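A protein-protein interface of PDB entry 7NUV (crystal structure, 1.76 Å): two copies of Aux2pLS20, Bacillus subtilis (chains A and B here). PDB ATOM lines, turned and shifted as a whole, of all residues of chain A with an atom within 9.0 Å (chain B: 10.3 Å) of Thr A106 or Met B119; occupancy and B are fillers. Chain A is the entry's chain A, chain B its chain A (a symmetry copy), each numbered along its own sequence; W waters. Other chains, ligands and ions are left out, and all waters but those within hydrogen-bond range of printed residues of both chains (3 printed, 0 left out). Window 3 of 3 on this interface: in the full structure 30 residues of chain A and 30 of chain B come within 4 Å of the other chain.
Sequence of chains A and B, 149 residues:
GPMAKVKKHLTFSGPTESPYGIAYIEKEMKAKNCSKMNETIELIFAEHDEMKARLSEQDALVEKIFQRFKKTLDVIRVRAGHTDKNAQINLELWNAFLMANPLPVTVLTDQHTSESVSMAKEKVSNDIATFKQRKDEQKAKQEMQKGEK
The backbone NH (N) of Ser B114 lies within hydrogen-bond range of the side-chain amide oxygen (OD1) of Asn A95, at 2.8 Å.
The side-chain hydroxyl (OG1) of Thr A106 lies within hydrogen-bond range of the side-chain hydroxyl (OG) of Ser B116, 2.6 Å away.
The side-chain amino group (NZ) of Lys B123 lies within hydrogen-bond range of the side-chain hydroxyl (OG1) of Thr A109.
OG of Ser B114 sits close to N of Ser B116 (3.3 Å).
The side-chain amino group (NZ) of Lys B123 is in salt-bridge range of the side-chain carboxylate (OD1) of Asp B127 (2.7 Å).
CA of Thr B113 touches OD1 of Asn A95, at 3.4 Å.
Val B117 touches Asn A95.
CB of Leu A98 touches OG of Ser B114, 3.9 Å away.
Leu A98 touches Ser B116 (CD1 to CB, 3.9 Å).
CD1 of Leu A103 touches OG of Ser B116 (3.8 Å).
O of Thr A106 touches CE of Met B119, at 3.8 Å.
Leu A108 touches Met B119.
CD1 of Leu A108 touches CB of Lys B123 (3.6 Å).
Asp A110 touches Lys B123.
Thr A106 touches just these residues of chain B: Ser B116 (2.6 Å) and Met B119 (3.8 Å).
Met B119 touches just these residues of chain A: Thr A106 and Leu A108.
Printed residues of chain B within 4 Å of Leu A103: Ser B116 (3.8 Å).
No residue of chain B comes within 4 Å of Val A105.
Val A107 touches none of the printed residues of chain B.
Leu A108 touches just these residues of chain B: Met B119 and Lys B123.
Printed residues of chain A within 4 Å of Val B117: Asn A95 (3.7 Å).
Of the printed residues of chain A, Thr B113 touches Asn A95 (3.4 Å).
Printed residues of chain B within 4 Å of Thr A109: Lys B123.
Of the printed residues of chain B, Asn A95 touches Thr B113 (3.4 Å), Ser B114 (2.8 Å) and Val B117 (3.7 Å).
Glu B115 touches none of the printed residues of chain A.
Asn B126 touches none of the printed residues of chain A.
The nearest printed residue of chain B that does not touch Leu A98 is Val B117 (4.6 Å).
Of the 15 printed residues of chain B, 6 touch a printed residue of chain A.
Printed residues of chain B that touch a printed residue of chain A: Thr B113, Ser B114, Ser B116, Val B117, Met B119 and Lys B123.
Hydrophobic or aromatic side chains of chain B that line the printed part of chain A: Val B117 and Met B119.
Among the printed residues, 12 pairs touch across the chains.
Among the printed residues, no Asp or Glu carboxylate lies within 4 Å of a Lys or Arg side-chain nitrogen of the other chain.
No position is printed for both chains.
Of the 12 pairs that touch across the chains among the printed residues, none has its exchanged pair printed and touching as well.
Water W1 bridges the side-chain hydroxyl of Ser B114 (2.6 Å) and the backbone carbonyl oxygen of Leu A98 (2.8 Å).
Water W3 lies within hydrogen-bond range of OG of Ser B116 (2.7 Å) and N of Leu A103 (2.9 Å).
Water W2 lies within hydrogen-bond range of the side-chain amino group of Lys B123 (2.7 Å) and the side-chain hydroxyl of Thr A109 (3.4 Å).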
ATOM      1  N   ASN A  95      -4.020  22.542  -1.241  1.00  0.00           N
ATOM      2  CA  ASN A  95      -3.107  21.772  -0.401  1.00  0.00           C
ATOM      3  C   ASN A  95      -1.657  22.126  -0.694  1.00  0.00           C
ATOM      4  O   ASN A  95      -0.877  22.386   0.225  1.00  0.00           O
ATOM      5  CB  ASN A  95      -3.320  20.274  -0.583  1.00  0.00           C
ATOM      6  CG  ASN A  95      -2.617  19.463   0.491  1.00  0.00           C
ATOM      7  OD1 ASN A  95      -3.105  19.389   1.622  1.00  0.00           O
ATOM      8  ND2 ASN A  95      -1.503  18.807   0.137  1.00  0.00           N
ATOM      9  N   LEU A  98      -0.935  25.823   0.383  1.00  0.00           N
ATOM     10  CA  LEU A  98      -0.818  25.978   1.828  1.00  0.00           C
ATOM     11  C   LEU A  98       0.347  25.179   2.389  1.00  0.00           C
ATOM     12  O   LEU A  98       0.900  25.555   3.429  1.00  0.00           O
ATOM     13  CB  LEU A  98      -2.135  25.587   2.506  1.00  0.00           C
ATOM     14  CG  LEU A  98      -3.304  26.538   2.261  1.00  0.00           C
ATOM     15  CD1 LEU A  98      -4.523  26.088   3.028  1.00  0.00           C
ATOM     16  CD2 LEU A  98      -2.922  27.936   2.737  1.00  0.00           C
ATOM     17  N   ASN A 101       3.021  27.653   1.768  1.00  0.00           N
ATOM     18  CA  ASN A 101       2.784  28.947   2.413  1.00  0.00           C
ATOM     19  C   ASN A 101       1.890  28.699   3.622  1.00  0.00           C
ATOM     20  O   ASN A 101       0.697  29.015   3.606  1.00  0.00           O
ATOM     21  CB  ASN A 101       2.125  29.910   1.422  1.00  0.00           C
ATOM     22  CG  ASN A 101       2.984  30.176   0.197  1.00  0.00           C
ATOM     23  OD1 ASN A 101       3.878  31.020   0.232  1.00  0.00           O
ATOM     24  ND2 ASN A 101       2.740  29.430  -0.882  1.00  0.00           N
ATOM     25  N   PRO A 102       2.422  28.080   4.670  1.00  0.00           N
ATOM     26  CA  PRO A 102       1.552  27.599   5.747  1.00  0.00           C
ATOM     27  C   PRO A 102       1.004  28.747   6.576  1.00  0.00           C
ATOM     28  O   PRO A 102       1.565  29.838   6.620  1.00  0.00           O
ATOM     29  CB  PRO A 102       2.458  26.688   6.579  1.00  0.00           C
ATOM     30  CG  PRO A 102       3.854  27.095   6.239  1.00  0.00           C
ATOM     31  CD  PRO A 102       3.841  27.751   4.886  1.00  0.00           C
ATOM     32  N   LEU A 103      -0.135  28.475   7.239  1.00  0.00           N
ATOM     33  CA  LEU A 103      -0.854  29.403   8.109  1.00  0.00           C
ATOM     34  C   LEU A 103      -0.416  29.191   9.555  1.00  0.00           C
ATOM     35  O   LEU A 103      -0.360  28.045  10.008  1.00  0.00           O
ATOM     36  CB  LEU A 103      -2.358  29.145   7.985  1.00  0.00           C
ATOM     37  CG  LEU A 103      -2.946  29.188   6.571  1.00  0.00           C
ATOM     38  CD1 LEU A 103      -4.471  29.114   6.643  1.00  0.00           C
ATOM     39  CD2 LEU A 103      -2.499  30.427   5.743  1.00  0.00           C
ATOM     40  N   PRO A 104      -0.070  30.247  10.306  1.00  0.00           N
ATOM     41  CA  PRO A 104       0.258  30.051  11.731  1.00  0.00           C
ATOM     42  C   PRO A 104      -0.905  29.513  12.541  1.00  0.00           C
ATOM     43  O   PRO A 104      -0.714  28.749  13.502  1.00  0.00           O
ATOM     44  CB  PRO A 104       0.634  31.464  12.201  1.00  0.00           C
ATOM     45  CG  PRO A 104       1.101  32.156  10.975  1.00  0.00           C
ATOM     46  CD  PRO A 104       0.265  31.599   9.838  1.00  0.00           C
ATOM     47  N   VAL A 105      -2.108  29.952  12.206  1.00  0.00           N
ATOM     48  CA  VAL A 105      -3.353  29.441  12.766  1.00  0.00           C
ATOM     49  C   VAL A 105      -4.342  29.303  11.611  1.00  0.00           C
ATOM     50  O   VAL A 105      -4.320  30.077  10.643  1.00  0.00           O
ATOM     51  CB  VAL A 105      -3.917  30.363  13.875  1.00  0.00           C
ATOM     52  CG1 VAL A 105      -2.825  30.851  14.807  1.00  0.00           C
ATOM     53  CG2 VAL A 105      -4.576  31.553  13.269  1.00  0.00           C
ATOM     54  N   THR A 106      -5.203  28.292  11.696  1.00  0.00           N
ATOM     55  CA  THR A 106      -6.227  28.049  10.684  1.00  0.00           C
ATOM     56  C   THR A 106      -7.575  28.421  11.294  1.00  0.00           C
ATOM     57  O   THR A 106      -8.089  27.695  12.154  1.00  0.00           O
ATOM     58  CB  THR A 106      -6.212  26.591  10.215  1.00  0.00           C
ATOM     59  OG1 THR A 106      -4.922  26.286   9.674  1.00  0.00           O
ATOM     60  CG2 THR A 106      -7.309  26.324   9.156  1.00  0.00           C
ATOM     61  N   VAL A 107      -8.135  29.548  10.864  1.00  0.00           N
ATOM     62  CA  VAL A 107      -9.362  30.086  11.447  1.00  0.00           C
ATOM     63  C   VAL A 107     -10.520  29.733  10.522  1.00  0.00           C
ATOM     64  O   VAL A 107     -10.623  30.261   9.415  1.00  0.00           O
ATOM     65  CB  VAL A 107      -9.268  31.601  11.673  1.00  0.00           C
ATOM     66  CG1 VAL A 107     -10.582  32.124  12.234  1.00  0.00           C
ATOM     67  CG2 VAL A 107      -8.159  31.914  12.661  1.00  0.00           C
ATOM     68  N   LEU A 108     -11.409  28.864  10.975  1.00  0.00           N
ATOM     69  CA  LEU A 108     -12.557  28.436  10.185  1.00  0.00           C
ATOM     70  C   LEU A 108     -13.761  29.317  10.507  1.00  0.00           C
ATOM     71  O   LEU A 108     -13.769  30.041  11.511  1.00  0.00           O
ATOM     72  CB  LEU A 108     -12.863  26.963  10.480  1.00  0.00           C
ATOM     73  CG  LEU A 108     -11.665  26.022  10.254  1.00  0.00           C
ATOM     74  CD1 LEU A 108     -12.092  24.588  10.435  1.00  0.00           C
ATOM     75  CD2 LEU A 108     -11.076  26.198   8.856  1.00  0.00           C
ATOM     76  N   THR A 109     -14.805  29.235   9.658  1.00  0.00           N
ATOM     77  CA  THR A 109     -15.889  30.210   9.751  1.00  0.00           C
ATOM     78  C   THR A 109     -16.717  30.009  11.010  1.00  0.00           C
ATOM     79  O   THR A 109     -17.455  30.922  11.406  1.00  0.00           O
ATOM     80  CB  THR A 109     -16.873  30.120   8.581  1.00  0.00           C
ATOM     81  OG1 THR A 109     -17.145  28.756   8.280  1.00  0.00           O
ATOM     82  CG2 THR A 109     -16.201  30.703   7.324  1.00  0.00           C
ATOM     83  N   ASP A 110     -16.665  28.821  11.620  1.00  0.00           N
ATOM     84  CA  ASP A 110     -17.382  28.664  12.879  1.00  0.00           C
ATOM     85  C   ASP A 110     -16.648  29.312  14.048  1.00  0.00           C
ATOM     86  O   ASP A 110     -17.225  29.434  15.132  1.00  0.00           O
ATOM     87  CB  ASP A 110     -17.663  27.188  13.219  1.00  0.00           C
ATOM     88  CG  ASP A 110     -16.423  26.290  13.180  1.00  0.00           C
ATOM     89  OD1 ASP A 110     -15.305  26.755  12.876  1.00  0.00           O
ATOM     90  OD2 ASP A 110     -16.578  25.080  13.488  1.00  0.00           O
ATOM     91  N   GLN A 111     -15.398  29.728  13.861  1.00  0.00           N
ATOM     92  CA  GLN A 111     -14.711  30.544  14.858  1.00  0.00           C
ATOM     93  C   GLN A 111     -14.839  32.029  14.552  1.00  0.00           C
ATOM     94  O   GLN A 111     -15.304  32.808  15.391  1.00  0.00           O
ATOM     95  CB  GLN A 111     -13.239  30.145  14.957  1.00  0.00           C
ATOM     96  CG  GLN A 111     -13.067  28.672  15.221  1.00  0.00           C
ATOM     97  CD  GLN A 111     -13.542  28.321  16.619  1.00  0.00           C
ATOM     98  OE1 GLN A 111     -13.278  29.053  17.579  1.00  0.00           O
ATOM     99  NE2 GLN A 111     -14.253  27.199  16.744  1.00  0.00           N
ATOM    100  N   HIS A 112     -14.418  32.431  13.357  1.00  0.00           N
ATOM    101  CA  HIS A 112     -14.537  33.809  12.893  1.00  0.00           C
ATOM    102  C   HIS A 112     -14.615  33.828  11.378  1.00  0.00           C
ATOM    103  O   HIS A 112     -13.803  33.181  10.719  1.00  0.00           O
ATOM    104  CB  HIS A 112     -13.351  34.650  13.375  1.00  0.00           C
ATOM    105  CG  HIS A 112     -13.592  36.121  13.276  1.00  0.00           C
ATOM    106  ND1 HIS A 112     -13.325  36.828  12.122  1.00  0.00           N
ATOM    107  CD2 HIS A 112     -14.164  37.000  14.131  1.00  0.00           C
ATOM    108  CE1 HIS A 112     -13.672  38.092  12.294  1.00  0.00           C
ATOM    109  NE2 HIS A 112     -14.190  38.221  13.501  1.00  0.00           N
ATOM    110  N   THR B 113      -1.257  15.819   3.545  1.00  0.00           N
ATOM    111  CA  THR B 113      -2.388  16.733   3.615  1.00  0.00           C
ATOM    112  C   THR B 113      -2.071  17.801   4.645  1.00  0.00           C
ATOM    113  O   THR B 113      -1.802  17.494   5.810  1.00  0.00           O
ATOM    114  CB  THR B 113      -3.697  16.019   3.960  1.00  0.00           C
ATOM    115  OG1 THR B 113      -4.000  15.056   2.946  1.00  0.00           O
ATOM    116  CG2 THR B 113      -4.881  17.018   4.033  1.00  0.00           C
ATOM    117  N   SER B 114      -2.079  19.043   4.188  1.00  0.00           N
ATOM    118  CA  SER B 114      -1.936  20.204   5.054  1.00  0.00           C
ATOM    119  C   SER B 114      -2.888  20.103   6.234  1.00  0.00           C
ATOM    120  O   SER B 114      -4.044  19.717   6.074  1.00  0.00           O
ATOM    121  CB  SER B 114      -2.242  21.464   4.244  1.00  0.00           C
ATOM    122  OG  SER B 114      -2.256  22.615   5.071  1.00  0.00           O
ATOM    123  N   GLU B 115      -2.415  20.465   7.431  1.00  0.00           N
ATOM    124  CA  GLU B 115      -3.341  20.466   8.556  1.00  0.00           C
ATOM    125  C   GLU B 115      -4.528  21.396   8.309  1.00  0.00           C
ATOM    126  O   GLU B 115      -5.630  21.113   8.780  1.00  0.00           O
ATOM    127  CB  GLU B 115      -2.657  20.898   9.842  1.00  0.00           C
ATOM    128  CG  GLU B 115      -1.962  19.797  10.584  1.00  0.00           C
ATOM    129  CD  GLU B 115      -1.353  20.314  11.874  1.00  0.00           C
ATOM    130  OE1 GLU B 115      -1.791  21.394  12.355  1.00  0.00           O
ATOM    131  OE2 GLU B 115      -0.399  19.680  12.365  1.00  0.00           O
ATOM    132  N   SER B 116      -4.323  22.515   7.600  1.00  0.00           N
ATOM    133  CA  SER B 116      -5.432  23.435   7.318  1.00  0.00           C
ATOM    134  C   SER B 116      -6.517  22.778   6.471  1.00  0.00           C
ATOM    135  O   SER B 116      -7.720  23.001   6.702  1.00  0.00           O
ATOM    136  CB  SER B 116      -4.926  24.713   6.625  1.00  0.00           C
ATOM    137  OG  SER B 116      -3.947  25.403   7.387  1.00  0.00           O
ATOM    138  N   VAL B 117      -6.109  22.000   5.462  1.00  0.00           N
ATOM    139  CA  VAL B 117      -7.044  21.247   4.632  1.00  0.00           C
ATOM    140  C   VAL B 117      -7.747  20.176   5.455  1.00  0.00           C
ATOM    141  O   VAL B 117      -8.969  20.004   5.371  1.00  0.00           O
ATOM    142  CB  VAL B 117      -6.302  20.645   3.421  1.00  0.00           C
ATOM    143  CG1 VAL B 117      -7.188  19.688   2.660  1.00  0.00           C
ATOM    144  CG2 VAL B 117      -5.871  21.759   2.475  1.00  0.00           C
ATOM    145  N   SER B 118      -6.995  19.458   6.278  1.00  0.00           N
ATOM    146  CA  SER B 118      -7.617  18.474   7.148  1.00  0.00           C
ATOM    147  C   SER B 118      -8.631  19.121   8.090  1.00  0.00           C
ATOM    148  O   SER B 118      -9.727  18.585   8.288  1.00  0.00           O
ATOM    149  CB  SER B 118      -6.539  17.730   7.930  1.00  0.00           C
ATOM    150  OG  SER B 118      -7.135  16.813   8.827  1.00  0.00           O
ATOM    151  N   MET B 119      -8.298  20.267   8.687  1.00  0.00           N
ATOM    152  CA  MET B 119      -9.283  20.866   9.590  1.00  0.00           C
ATOM    153  C   MET B 119     -10.518  21.347   8.846  1.00  0.00           C
ATOM    154  O   MET B 119     -11.637  21.254   9.375  1.00  0.00           O
ATOM    155  CB  MET B 119      -8.712  22.021  10.436  1.00  0.00           C
ATOM    156  CG  MET B 119      -7.662  21.655  11.480  1.00  0.00           C
ATOM    157  SD  MET B 119      -6.519  23.001  11.915  1.00  0.00           S
ATOM    158  CE  MET B 119      -7.622  23.998  12.927  1.00  0.00           C
ATOM    159  N   ALA B 120     -10.343  21.902   7.642  1.00  0.00           N
ATOM    160  CA  ALA B 120     -11.496  22.328   6.860  1.00  0.00           C
ATOM    161  C   ALA B 120     -12.374  21.141   6.483  1.00  0.00           C
ATOM    162  O   ALA B 120     -13.611  21.244   6.493  1.00  0.00           O
ATOM    163  CB  ALA B 120     -11.042  23.080   5.603  1.00  0.00           C
ATOM    164  N   LYS B 121     -11.766  20.014   6.120  1.00  0.00           N
ATOM    165  CA  LYS B 121     -12.559  18.847   5.752  1.00  0.00           C
ATOM    166  C   LYS B 121     -13.344  18.317   6.943  1.00  0.00           C
ATOM    167  O   LYS B 121     -14.499  17.900   6.790  1.00  0.00           O
ATOM    168  CB  LYS B 121     -11.653  17.757   5.173  1.00  0.00           C
ATOM    169  CG  LYS B 121     -11.017  18.147   3.831  1.00  0.00           C
ATOM    170  CD  LYS B 121     -10.136  17.045   3.226  1.00  0.00           C
ATOM    171  CE  LYS B 121     -10.533  15.656   3.692  1.00  0.00           C
ATOM    172  NZ  LYS B 121      -9.644  14.611   3.099  1.00  0.00           N
ATOM    173  N   GLU B 122     -12.734  18.315   8.134  1.00  0.00           N
ATOM    174  CA  GLU B 122     -13.444  17.836   9.313  1.00  0.00           C
ATOM    175  C   GLU B 122     -14.586  18.786   9.671  1.00  0.00           C
ATOM    176  O   GLU B 122     -15.682  18.344  10.034  1.00  0.00           O
ATOM    177  CB  GLU B 122     -12.499  17.704  10.505  1.00  0.00           C
ATOM    178  CG  GLU B 122     -11.454  16.596  10.365  1.00  0.00           C
ATOM    179  CD  GLU B 122     -11.985  15.189  10.553  1.00  0.00           C
ATOM    180  OE1 GLU B 122     -13.195  15.011  10.781  1.00  0.00           O
ATOM    181  OE2 GLU B 122     -11.164  14.247  10.466  1.00  0.00           O
ATOM    182  N   LYS B 123     -14.349  20.092   9.577  1.00  0.00           N
ATOM    183  CA  LYS B 123     -15.407  21.039   9.912  1.00  0.00           C
ATOM    184  C   LYS B 123     -16.606  20.849   8.989  1.00  0.00           C
ATOM    185  O   LYS B 123     -17.758  20.798   9.438  1.00  0.00           O
ATOM    186  CB  LYS B 123     -14.919  22.476   9.781  1.00  0.00           C
ATOM    187  CG  LYS B 123     -15.965  23.397  10.337  1.00  0.00           C
ATOM    188  CD  LYS B 123     -16.226  24.586   9.465  1.00  0.00           C
ATOM    189  CE  LYS B 123     -17.534  25.219   9.938  1.00  0.00           C
ATOM    190  NZ  LYS B 123     -18.301  25.847   8.860  1.00  0.00           N
ATOM    191  N   VAL B 124     -16.351  20.774   7.682  1.00  0.00           N
ATOM    192  CA  VAL B 124     -17.447  20.624   6.730  1.00  0.00           C
ATOM    193  C   VAL B 124     -18.112  19.253   6.890  1.00  0.00           C
ATOM    194  O   VAL B 124     -19.342  19.137   6.843  1.00  0.00           O
ATOM    195  CB  VAL B 124     -16.941  20.864   5.294  1.00  0.00           C
ATOM    196  CG1 VAL B 124     -18.007  20.478   4.273  1.00  0.00           C
ATOM    197  CG2 VAL B 124     -16.499  22.319   5.112  1.00  0.00           C
ATOM    198  N   SER B 125     -17.328  18.201   7.125  1.00  0.00           N
ATOM    199  CA  SER B 125     -17.926  16.892   7.378  1.00  0.00           C
ATOM    200  C   SER B 125     -18.894  16.941   8.560  1.00  0.00           C
ATOM    201  O   SER B 125     -19.968  16.332   8.519  1.00  0.00           O
ATOM    202  CB  SER B 125     -16.841  15.855   7.643  1.00  0.00           C
ATOM    203  OG  SER B 125     -16.153  15.523   6.460  1.00  0.00           O
ATOM    204  N   ASN B 126     -18.528  17.648   9.622  1.00  0.00           N
ATOM    205  CA  ASN B 126     -19.410  17.756  10.775  1.00  0.00           C
ATOM    206  C   ASN B 126     -20.605  18.649  10.467  1.00  0.00           C
ATOM    207  O   ASN B 126     -21.698  18.414  10.984  1.00  0.00           O
ATOM    208  CB  ASN B 126     -18.618  18.266  11.980  1.00  0.00           C
ATOM    209  CG  ASN B 126     -17.665  17.207  12.527  1.00  0.00           C
ATOM    210  OD1 ASN B 126     -17.987  16.022  12.517  1.00  0.00           O
ATOM    211  ND2 ASN B 126     -16.493  17.626  13.002  1.00  0.00           N
ATOM    212  N   ASP B 127     -20.425  19.651   9.602  1.00  0.00           N
ATOM    213  CA  ASP B 127     -21.531  20.536   9.242  1.00  0.00           C
ATOM    214  C   ASP B 127     -22.612  19.735   8.539  1.00  0.00           C
ATOM    215  O   ASP B 127     -23.813  19.878   8.815  1.00  0.00           O
ATOM    216  CB  ASP B 127     -21.058  21.625   8.276  1.00  0.00           C
ATOM    217  CG  ASP B 127     -20.458  22.844   8.964  1.00  0.00           C
ATOM    218  OD1 ASP B 127     -19.716  23.578   8.261  1.00  0.00           O
ATOM    219  OD2 ASP B 127     -20.599  22.999  10.195  1.00  0.00           O
HETATM  220  O   HOH W   1      -0.125  24.022   5.571  1.00  0.00           O
HETATM  221  O   HOH W   2     -19.883  27.775   9.949  1.00  0.00           O
HETATM  222  O   HOH W   3      -1.257  25.769   7.245  1.00  0.00           O
